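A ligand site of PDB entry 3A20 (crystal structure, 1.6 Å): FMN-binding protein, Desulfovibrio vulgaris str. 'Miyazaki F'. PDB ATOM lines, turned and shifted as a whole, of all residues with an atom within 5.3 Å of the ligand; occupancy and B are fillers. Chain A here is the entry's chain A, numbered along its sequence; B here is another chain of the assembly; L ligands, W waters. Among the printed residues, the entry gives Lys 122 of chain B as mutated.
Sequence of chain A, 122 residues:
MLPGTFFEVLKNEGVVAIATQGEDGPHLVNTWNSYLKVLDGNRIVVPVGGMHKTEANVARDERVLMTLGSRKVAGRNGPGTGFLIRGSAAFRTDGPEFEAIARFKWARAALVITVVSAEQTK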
ATOM      1  N   VAL A  15      23.210   2.302 -12.082  1.00  0.00           N
ATOM      2  CA  VAL A  15      22.272   1.524 -12.869  1.00  0.00           C
ATOM      3  C   VAL A  15      22.190   0.088 -12.349  1.00  0.00           C
ATOM      4  O   VAL A  15      23.196  -0.610 -12.248  1.00  0.00           O
ATOM      5  CB  VAL A  15      22.689   1.507 -14.356  1.00  0.00           C
ATOM      6  CG1 VAL A  15      21.769   0.603 -15.168  1.00  0.00           C
ATOM      7  CG2 VAL A  15      22.660   2.928 -14.902  1.00  0.00           C
ATOM      8  N   HIS A  27      16.621 -12.195 -20.460  1.00  0.00           N
ATOM      9  CA  HIS A  27      16.121 -10.856 -20.728  1.00  0.00           C
ATOM     10  C   HIS A  27      16.788 -10.010 -19.653  1.00  0.00           C
ATOM     11  O   HIS A  27      17.103 -10.503 -18.568  1.00  0.00           O
ATOM     12  CB  HIS A  27      14.602 -10.743 -20.626  1.00  0.00           C
ATOM     13  CG  HIS A  27      14.078  -9.430 -21.111  1.00  0.00           C
ATOM     14  ND1 HIS A  27      14.454  -8.888 -22.326  1.00  0.00           N
ATOM     15  CD2 HIS A  27      13.247  -8.526 -20.540  1.00  0.00           C
ATOM     16  CE1 HIS A  27      13.872  -7.709 -22.478  1.00  0.00           C
ATOM     17  NE2 HIS A  27      13.133  -7.463 -21.411  1.00  0.00           N
ATOM     18  N   VAL A  29      16.682  -5.961 -17.881  1.00  0.00           N
ATOM     19  CA  VAL A  29      16.112  -4.624 -17.768  1.00  0.00           C
ATOM     20  C   VAL A  29      16.806  -3.874 -16.641  1.00  0.00           C
ATOM     21  O   VAL A  29      17.612  -4.441 -15.895  1.00  0.00           O
ATOM     22  CB  VAL A  29      14.594  -4.654 -17.495  1.00  0.00           C
ATOM     23  CG1 VAL A  29      13.871  -5.305 -18.663  1.00  0.00           C
ATOM     24  CG2 VAL A  29      14.291  -5.378 -16.186  1.00  0.00           C
ATOM     25  N   ASN A  30      16.491  -2.590 -16.484  1.00  0.00           N
ATOM     26  CA  ASN A  30      17.146  -1.788 -15.470  1.00  0.00           C
ATOM     27  C   ASN A  30      16.233  -0.946 -14.596  1.00  0.00           C
ATOM     28  O   ASN A  30      15.041  -0.834 -14.843  1.00  0.00           O
ATOM     29  CB  ASN A  30      18.115  -0.801 -16.132  1.00  0.00           C
ATOM     30  CG  ASN A  30      19.104  -1.468 -17.036  1.00  0.00           C
ATOM     31  OD1 ASN A  30      18.996  -1.386 -18.266  1.00  0.00           O
ATOM     32  ND2 ASN A  30      20.077  -2.146 -16.452  1.00  0.00           N
ATOM     33  N   THR A  31      16.852  -0.372 -13.573  1.00  0.00           N
ATOM     34  CA  THR A  31      16.247   0.585 -12.661  1.00  0.00           C
ATOM     35  C   THR A  31      17.435   1.350 -12.090  1.00  0.00           C
ATOM     36  O   THR A  31      18.568   1.130 -12.531  1.00  0.00           O
ATOM     37  CB  THR A  31      15.387  -0.028 -11.527  1.00  0.00           C
ATOM     38  OG1 THR A  31      14.712   1.039 -10.842  1.00  0.00           O
ATOM     39  CG2 THR A  31      16.238  -0.794 -10.533  1.00  0.00           C
ATOM     40  N   TRP A  32      17.193   2.243 -11.140  1.00  0.00           N
ATOM     41  CA  TRP A  32      18.267   3.026 -10.536  1.00  0.00           C
ATOM     42  C   TRP A  32      18.544   2.630  -9.101  1.00  0.00           C
ATOM     43  O   TRP A  32      17.645   2.194  -8.383  1.00  0.00           O
ATOM     44  CB  TRP A  32      17.929   4.520 -10.551  1.00  0.00           C
ATOM     45  CG  TRP A  32      17.678   5.112 -11.907  1.00  0.00           C
ATOM     46  CD1 TRP A  32      16.467   5.329 -12.493  1.00  0.00           C
ATOM     47  CD2 TRP A  32      18.659   5.613 -12.815  1.00  0.00           C
ATOM     48  NE1 TRP A  32      16.630   5.945 -13.707  1.00  0.00           N
ATOM     49  CE2 TRP A  32      17.971   6.131 -13.930  1.00  0.00           C
ATOM     50  CE3 TRP A  32      20.058   5.670 -12.795  1.00  0.00           C
ATOM     51  CZ2 TRP A  32      18.632   6.707 -15.025  1.00  0.00           C
ATOM     52  CZ3 TRP A  32      20.720   6.243 -13.881  1.00  0.00           C
ATOM     53  CH2 TRP A  32      19.999   6.753 -14.981  1.00  0.00           C
ATOM     54  N   TYR A  35      16.213   4.090  -6.697  1.00  0.00           N
ATOM     55  CA  TYR A  35      14.822   3.664  -6.744  1.00  0.00           C
ATOM     56  C   TYR A  35      14.543   2.443  -5.877  1.00  0.00           C
ATOM     57  O   TYR A  35      13.397   2.190  -5.503  1.00  0.00           O
ATOM     58  CB  TYR A  35      14.386   3.333  -8.169  1.00  0.00           C
ATOM     59  CG  TYR A  35      14.093   4.514  -9.073  1.00  0.00           C
ATOM     60  CD1 TYR A  35      13.439   4.323 -10.290  1.00  0.00           C
ATOM     61  CD2 TYR A  35      14.462   5.817  -8.724  1.00  0.00           C
ATOM     62  CE1 TYR A  35      13.150   5.388 -11.134  1.00  0.00           C
ATOM     63  CE2 TYR A  35      14.175   6.895  -9.563  1.00  0.00           C
ATOM     64  CZ  TYR A  35      13.517   6.673 -10.759  1.00  0.00           C
ATOM     65  OH  TYR A  35      13.221   7.728 -11.594  1.00  0.00           O
ATOM     66  N   VAL A  46      11.121  -2.696  -6.484  1.00  0.00           N
ATOM     67  CA  VAL A  46      11.426  -1.857  -7.632  1.00  0.00           C
ATOM     68  C   VAL A  46      10.144  -1.279  -8.236  1.00  0.00           C
ATOM     69  O   VAL A  46       9.173  -1.997  -8.445  1.00  0.00           O
ATOM     70  CB  VAL A  46      12.128  -2.684  -8.731  1.00  0.00           C
ATOM     71  CG1 VAL A  46      12.404  -1.813  -9.948  1.00  0.00           C
ATOM     72  CG2 VAL A  46      13.425  -3.292  -8.198  1.00  0.00           C
ATOM     73  N   PRO A  47      10.129   0.038  -8.520  1.00  0.00           N
ATOM     74  CA  PRO A  47       8.933   0.633  -9.113  1.00  0.00           C
ATOM     75  C   PRO A  47       8.837   0.175 -10.567  1.00  0.00           C
ATOM     76  O   PRO A  47       9.795   0.291 -11.326  1.00  0.00           O
ATOM     77  CB  PRO A  47       9.191   2.137  -8.986  1.00  0.00           C
ATOM     78  CG  PRO A  47      10.687   2.228  -9.084  1.00  0.00           C
ATOM     79  CD  PRO A  47      11.145   1.064  -8.232  1.00  0.00           C
ATOM     80  N   VAL A  48       7.670  -0.351 -10.951  1.00  0.00           N
ATOM     81  CA  VAL A  48       7.477  -0.860 -12.306  1.00  0.00           C
ATOM     82  C   VAL A  48       6.630   0.043 -13.198  1.00  0.00           C
ATOM     83  O   VAL A  48       5.458   0.286 -12.915  1.00  0.00           O
ATOM     84  CB  VAL A  48       6.840  -2.268 -12.264  1.00  0.00           C
ATOM     85  CG1 VAL A  48       6.596  -2.765 -13.681  1.00  0.00           C
ATOM     86  CG2 VAL A  48       7.741  -3.229 -11.509  1.00  0.00           C
ATOM     87  N   GLY A  49       7.247   0.506 -14.276  1.00  0.00           N
ATOM     88  CA  GLY A  49       6.546   1.336 -15.254  1.00  0.00           C
ATOM     89  C   GLY A  49       6.257   0.422 -16.429  1.00  0.00           C
ATOM     90  O   GLY A  49       5.099   0.189 -16.778  1.00  0.00           O
ATOM     91  N   GLY A  50       7.318  -0.110 -17.024  1.00  0.00           N
ATOM     92  CA  GLY A  50       7.185  -1.026 -18.135  1.00  0.00           C
ATOM     93  C   GLY A  50       7.314  -2.460 -17.649  1.00  0.00           C
ATOM     94  O   GLY A  50       6.387  -2.996 -17.056  1.00  0.00           O
ATOM     95  N   MET A  51       8.471  -3.064 -17.907  1.00  0.00           N
ATOM     96  CA  MET A  51       8.759  -4.436 -17.484  1.00  0.00           C
ATOM     97  C   MET A  51       7.655  -5.459 -17.774  1.00  0.00           C
ATOM     98  O   MET A  51       7.358  -6.321 -16.948  1.00  0.00           O
ATOM     99  CB  MET A  51       9.102  -4.466 -15.994  1.00  0.00           C
ATOM    100  CG  MET A  51      10.322  -3.628 -15.665  1.00  0.00           C
ATOM    101  SD  MET A  51      10.977  -3.992 -14.033  1.00  0.00           S
ATOM    102  CE  MET A  51      12.351  -2.887 -13.977  1.00  0.00           C
ATOM    103  N   HIS A  52       7.070  -5.353 -18.956  1.00  0.00           N
ATOM    104  CA  HIS A  52       6.014  -6.273 -19.356  1.00  0.00           C
ATOM    105  C   HIS A  52       6.613  -7.613 -19.777  1.00  0.00           C
ATOM    106  O   HIS A  52       6.071  -8.672 -19.449  1.00  0.00           O
ATOM    107  CB  HIS A  52       5.194  -5.670 -20.506  1.00  0.00           C
ATOM    108  CG  HIS A  52       4.349  -4.504 -20.085  1.00  0.00           C
ATOM    109  ND1 HIS A  52       3.261  -4.639 -19.250  1.00  0.00           N
ATOM    110  CD2 HIS A  52       4.452  -3.180 -20.369  1.00  0.00           C
ATOM    111  CE1 HIS A  52       2.732  -3.441 -19.040  1.00  0.00           C
ATOM    112  NE2 HIS A  52       3.434  -2.545 -19.706  1.00  0.00           N
ATOM    113  N   LYS A  53       7.736  -7.594 -20.491  1.00  0.00           N
ATOM    114  CA  LYS A  53       8.375  -8.834 -20.910  1.00  0.00           C
ATOM    115  C   LYS A  53       8.959  -9.499 -19.658  1.00  0.00           C
ATOM    116  O   LYS A  53       8.893 -10.722 -19.494  1.00  0.00           O
ATOM    117  CB  LYS A  53       9.489  -8.558 -21.923  1.00  0.00           C
ATOM    118  CG  LYS A  53       9.053  -7.777 -23.134  1.00  0.00           C
ATOM    119  CD  LYS A  53      10.213  -7.588 -24.105  1.00  0.00           C
ATOM    120  CE  LYS A  53      10.297  -6.128 -24.571  1.00  0.00           C
ATOM    121  NZ  LYS A  53      11.644  -5.527 -24.316  1.00  0.00           N
ATOM    122  N   THR A  54       9.521  -8.672 -18.780  1.00  0.00           N
ATOM    123  CA  THR A  54      10.091  -9.161 -17.537  1.00  0.00           C
ATOM    124  C   THR A  54       9.009  -9.840 -16.695  1.00  0.00           C
ATOM    125  O   THR A  54       9.221 -10.928 -16.167  1.00  0.00           O
ATOM    126  CB  THR A  54      10.738  -8.012 -16.738  1.00  0.00           C
ATOM    127  OG1 THR A  54      11.842  -7.496 -17.489  1.00  0.00           O
ATOM    128  CG2 THR A  54      11.222  -8.482 -15.380  1.00  0.00           C
ATOM    129  N   GLU A  55       7.840  -9.215 -16.603  1.00  0.00           N
ATOM    130  CA  GLU A  55       6.744  -9.779 -15.831  1.00  0.00           C
ATOM    131  C   GLU A  55       6.284 -11.113 -16.429  1.00  0.00           C
ATOM    132  O   GLU A  55       5.953 -12.052 -15.706  1.00  0.00           O
ATOM    133  CB  GLU A  55       5.557  -8.799 -15.749  1.00  0.00           C
ATOM    134  CG  GLU A  55       4.414  -9.324 -14.893  1.00  0.00           C
ATOM    135  CD  GLU A  55       3.315  -8.316 -14.651  1.00  0.00           C
ATOM    136  OE1 GLU A  55       3.310  -7.242 -15.309  1.00  0.00           O
ATOM    137  OE2 GLU A  55       2.438  -8.592 -13.801  1.00  0.00           O
ATOM    138  N   TRP A 106       4.105   6.913 -11.825  1.00  0.00           N
ATOM    139  CA  TRP A 106       4.114   6.232 -13.099  1.00  0.00           C
ATOM    140  C   TRP A 106       4.180   4.718 -12.911  1.00  0.00           C
ATOM    141  O   TRP A 106       4.096   3.956 -13.866  1.00  0.00           O
ATOM    142  CB  TRP A 106       5.320   6.686 -13.943  1.00  0.00           C
ATOM    143  CG  TRP A 106       6.613   6.745 -13.177  1.00  0.00           C
ATOM    144  CD1 TRP A 106       7.163   7.852 -12.597  1.00  0.00           C
ATOM    145  CD2 TRP A 106       7.513   5.657 -12.910  1.00  0.00           C
ATOM    146  NE1 TRP A 106       8.348   7.529 -11.984  1.00  0.00           N
ATOM    147  CE2 TRP A 106       8.593   6.190 -12.160  1.00  0.00           C
ATOM    148  CE3 TRP A 106       7.513   4.299 -13.230  1.00  0.00           C
ATOM    149  CZ2 TRP A 106       9.660   5.400 -11.734  1.00  0.00           C
ATOM    150  CZ3 TRP A 106       8.580   3.509 -12.804  1.00  0.00           C
ATOM    151  CH2 TRP A 106       9.645   4.064 -12.063  1.00  0.00           C
ATOM    152  N   LEU B  68      23.769  -0.647 -19.676  1.00  0.00           N
ATOM    153  CA  LEU B  68      24.615   0.349 -19.041  1.00  0.00           C
ATOM    154  C   LEU B  68      23.885   1.677 -19.142  1.00  0.00           C
ATOM    155  O   LEU B  68      22.938   1.809 -19.923  1.00  0.00           O
ATOM    156  CB  LEU B  68      25.975   0.449 -19.750  1.00  0.00           C
ATOM    157  CG  LEU B  68      26.048   1.140 -21.112  1.00  0.00           C
ATOM    158  CD1 LEU B  68      27.504   1.454 -21.449  1.00  0.00           C
ATOM    159  CD2 LEU B  68      25.422   0.253 -22.180  1.00  0.00           C
ATOM    160  N   GLY B  69      24.302   2.650 -18.346  1.00  0.00           N
ATOM    161  CA  GLY B  69      23.650   3.948 -18.388  1.00  0.00           C
ATOM    162  C   GLY B  69      24.349   4.965 -17.512  1.00  0.00           C
ATOM    163  O   GLY B  69      25.423   4.704 -16.982  1.00  0.00           O
ATOM    164  N   THR B  81      19.824   8.144 -18.575  1.00  0.00           N
ATOM    165  CA  THR B  81      19.461   7.273 -19.683  1.00  0.00           C
ATOM    166  C   THR B  81      20.304   6.018 -19.653  1.00  0.00           C
ATOM    167  O   THR B  81      21.219   5.892 -18.829  1.00  0.00           O
ATOM    168  CB  THR B  81      19.637   7.976 -21.050  1.00  0.00           C
ATOM    169  OG1 THR B  81      19.052   7.163 -22.074  1.00  0.00           O
ATOM    170  CG2 THR B  81      21.112   8.173 -21.353  1.00  0.00           C
ATOM    171  N   GLY B  82      20.006   5.082 -20.547  1.00  0.00           N
ATOM    172  CA  GLY B  82      20.754   3.851 -20.609  1.00  0.00           C
ATOM    173  C   GLY B  82      20.383   3.076 -21.840  1.00  0.00           C
ATOM    174  O   GLY B  82      19.468   3.467 -22.571  1.00  0.00           O
ATOM    175  N   PHE B  83      21.071   1.952 -22.064  1.00  0.00           N
ATOM    176  CA  PHE B  83      20.856   1.141 -23.245  1.00  0.00           C
ATOM    177  C   PHE B  83      20.796  -0.357 -23.013  1.00  0.00           C
ATOM    178  O   PHE B  83      21.407  -0.884 -22.073  1.00  0.00           O
ATOM    179  CB  PHE B  83      21.980   1.368 -24.259  1.00  0.00           C
ATOM    180  CG  PHE B  83      22.018   2.749 -24.815  1.00  0.00           C
ATOM    181  CD1 PHE B  83      22.564   3.808 -24.088  1.00  0.00           C
ATOM    182  CD2 PHE B  83      21.493   3.006 -26.078  1.00  0.00           C
ATOM    183  CE1 PHE B  83      22.576   5.100 -24.599  1.00  0.00           C
ATOM    184  CE2 PHE B  83      21.494   4.295 -26.599  1.00  0.00           C
ATOM    185  CZ  PHE B  83      22.040   5.337 -25.868  1.00  0.00           C
ATOM    186  N   THR B 121      16.723   2.696 -23.728  1.00  0.00           N
ATOM    187  CA  THR B 121      15.529   2.324 -22.984  1.00  0.00           C
ATOM    188  C   THR B 121      14.960   3.342 -21.987  1.00  0.00           C
ATOM    189  O   THR B 121      14.104   3.004 -21.169  1.00  0.00           O
ATOM    190  CB  THR B 121      15.763   0.992 -22.277  1.00  0.00           C
ATOM    191  OG1 THR B 121      16.989   1.063 -21.547  1.00  0.00           O
ATOM    192  CG2 THR B 121      15.866  -0.144 -23.301  1.00  0.00           C
ATOM    193  N   LYS B 122      15.440   4.577 -22.058  1.00  0.00           N
ATOM    194  CA  LYS B 122      14.941   5.652 -21.208  1.00  0.00           C
ATOM    195  C   LYS B 122      15.190   6.994 -21.893  1.00  0.00           C
ATOM    196  O   LYS B 122      16.271   7.128 -22.504  1.00  0.00           O
ATOM    197  CB  LYS B 122      15.630   5.652 -19.836  1.00  0.00           C
ATOM    198  CG  LYS B 122      15.106   6.772 -18.927  1.00  0.00           C
ATOM    199  CD  LYS B 122      15.916   6.910 -17.656  1.00  0.00           C
ATOM    200  CE  LYS B 122      15.352   8.022 -16.786  1.00  0.00           C
ATOM    201  NZ  LYS B 122      15.286   9.342 -17.490  1.00  0.00           N
ATOM    202  OXT LYS B 122      14.314   7.882 -21.797  1.00  0.00           O
HETATM  203  N1  LIG L   1      11.623   0.519 -16.191  1.00  0.00           N
HETATM  204  C1  LIG L   1      10.751   0.417 -15.135  1.00  0.00           C
HETATM  205  O1  LIG L   1       9.667  -0.138 -15.249  1.00  0.00           O
HETATM  206  N2  LIG L   1      11.147   0.946 -13.881  1.00  0.00           N
HETATM  207  C2  LIG L   1      12.341   1.571 -13.627  1.00  0.00           C
HETATM  208  O2  LIG L   1      12.611   2.015 -12.484  1.00  0.00           O
HETATM  209  C3  LIG L   1      13.269   1.690 -14.756  1.00  0.00           C
HETATM  210  N3  LIG L   1      14.471   2.297 -14.578  1.00  0.00           N
HETATM  211  C4  LIG L   1      15.367   2.350 -15.639  1.00  0.00           C
HETATM  212  C5  LIG L   1      16.656   2.936 -15.456  1.00  0.00           C
HETATM  213  C6  LIG L   1      17.596   3.010 -16.495  1.00  0.00           C
HETATM  214  C7  LIG L   1      18.943   3.629 -16.244  1.00  0.00           C
HETATM  215  C8  LIG L   1      17.213   2.484 -17.784  1.00  0.00           C
HETATM  216  C9  LIG L   1      18.211   2.546 -18.963  1.00  0.00           C
HETATM  217  C10 LIG L   1      15.974   1.915 -17.981  1.00  0.00           C
HETATM  218  C11 LIG L   1      15.007   1.811 -16.949  1.00  0.00           C
HETATM  219  N4  LIG L   1      13.720   1.216 -17.092  1.00  0.00           N
HETATM  220  C12 LIG L   1      12.835   1.127 -16.004  1.00  0.00           C
HETATM  221  C13 LIG L   1      13.287   0.621 -18.376  1.00  0.00           C
HETATM  222  C14 LIG L   1      13.526  -0.910 -18.334  1.00  0.00           C
HETATM  223  O3  LIG L   1      14.915  -1.201 -18.329  1.00  0.00           O
HETATM  224  C15 LIG L   1      12.848  -1.644 -19.492  1.00  0.00           C
HETATM  225  O4  LIG L   1      13.461  -1.192 -20.719  1.00  0.00           O
HETATM  226  C16 LIG L   1      11.340  -1.418 -19.588  1.00  0.00           C
HETATM  227  O5  LIG L   1      10.669  -1.433 -18.303  1.00  0.00           O
HETATM  228  C17 LIG L   1      10.683  -2.476 -20.457  1.00  0.00           C
HETATM  229  O6  LIG L   1      10.746  -3.739 -19.760  1.00  0.00           O
HETATM  230  P1  LIG L   1      10.555  -5.112 -20.578  1.00  0.00           P
HETATM  231  O7  LIG L   1      11.631  -5.156 -21.643  1.00  0.00           O
HETATM  232  O8  LIG L   1       9.161  -5.081 -21.205  1.00  0.00           O
HETATM  233  O9  LIG L   1      10.670  -6.181 -19.532  1.00  0.00           O
HETATM  234  O   HOH W   1       7.276  -3.157 -21.263  1.00  0.00           O
HETATM  235  O   HOH W   2      12.103   0.768 -22.398  1.00  0.00           O
HETATM  236  O   HOH W   3      13.646  -3.484 -22.248  1.00  0.00           O
HETATM  237  O   HOH W   4       9.304   3.026 -16.592  1.00  0.00           O
HETATM  238  O   HOH W   5      16.979  -1.111 -20.073  1.00  0.00           O
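CG1 of Val 29 touches O9 of the ligand (3.4 Å). CZ2 of Trp 32 touches C7 of the ligand, at 3.3 Å. CD1 of Tyr 35 touches O2 of the ligand (3.3 Å). Val 48 touches the ligand. Trp 106 touches the ligand (CH2 to O2, 3.6 Å). Gly 82 of chain B touches the ligand. Thr 121 of chain B touches the ligand (OG1 to C9, 3.2 Å). Hydrophobic or aromatic side chains within 4 Å of the ligand: His 27, Val 29, Trp 32, Tyr 35, Pro 47, Met 51 and Trp 106. 17 residues have an atom within 4 Å of the ligand: His 27, Val 29, Asn 30, Thr 31, Trp 32, Tyr 35, Pro 47, Val 48, Gly 49, Gly 50, Met 51, His 52, Lys 53, Thr 54, Trp 106, Gly 82 of chain B and Thr 121 of chain B. Along chain A the residues within 4 Å of the ligand span positions 27 to 106.
An oxygen (O8) of the ligand is in hydrogen-bond range of the backbone NH (N) of His 52, at 3.1 Å. The backbone carbonyl oxygen (O) of Pro 47 lies within hydrogen-bond range of a nitrogen (N2) of the ligand (3.0 Å). The side-chain hydroxyl (OG1) of Thr 54 sits at hydrogen-bond distance from an oxygen (O9) of the ligand, at 2.7 Å. N of Gly 50 sits at hydrogen-bond distance from O1 of the ligand. The backbone NH (N) of Thr 54 is in hydrogen-bond range of an oxygen (O9) of the ligand, 2.8 Å away. An oxygen (O2) of the ligand is in hydrogen-bond range of the side-chain hydroxyl (OG1) of Thr 31 (2.8 Å). The backbone NH (N) of Met 51 is in hydrogen-bond range of an oxygen (O5) of the ligand (2.8 Å). N of Gly 49 lies within hydrogen-bond range of O1 of the ligand. NE2 of His 27 is in hydrogen-bond range of O7 of the ligand (2.8 Å). O7 of the ligand lies within salt-bridge range of NZ of Lys 53, at 2.7 Å. The backbone NH (N) of Lys 53 lies within hydrogen-bond range of an oxygen (O8) of the ligand, 3.0 Å away. The backbone NH (N) of Asn 30 is in hydrogen-bond range of an oxygen (O3) of the ligand (2.8 Å).
The backbone NH (N) of Thr 121 of chain B lies within hydrogen-bond range of the backbone carbonyl oxygen (O) of Gly 82 of chain B (3.1 Å).
Water W1 bridges an oxygen (O8) of the ligand (2.7 Å) and the backbone NH of His 52 (3.2 Å). Water W5 lies within hydrogen-bond range of the side-chain hydroxyl of Thr 121 of chain B (2.6 Å), an oxygen (O3) of the ligand (2.7 Å) and the side-chain amide oxygen of Asn 30 (2.7 Å). Water W2 bridges an oxygen (O4) of the ligand (2.9 Å) and the backbone carbonyl oxygen (O) of Thr 121 of chain B (3.2 Å).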
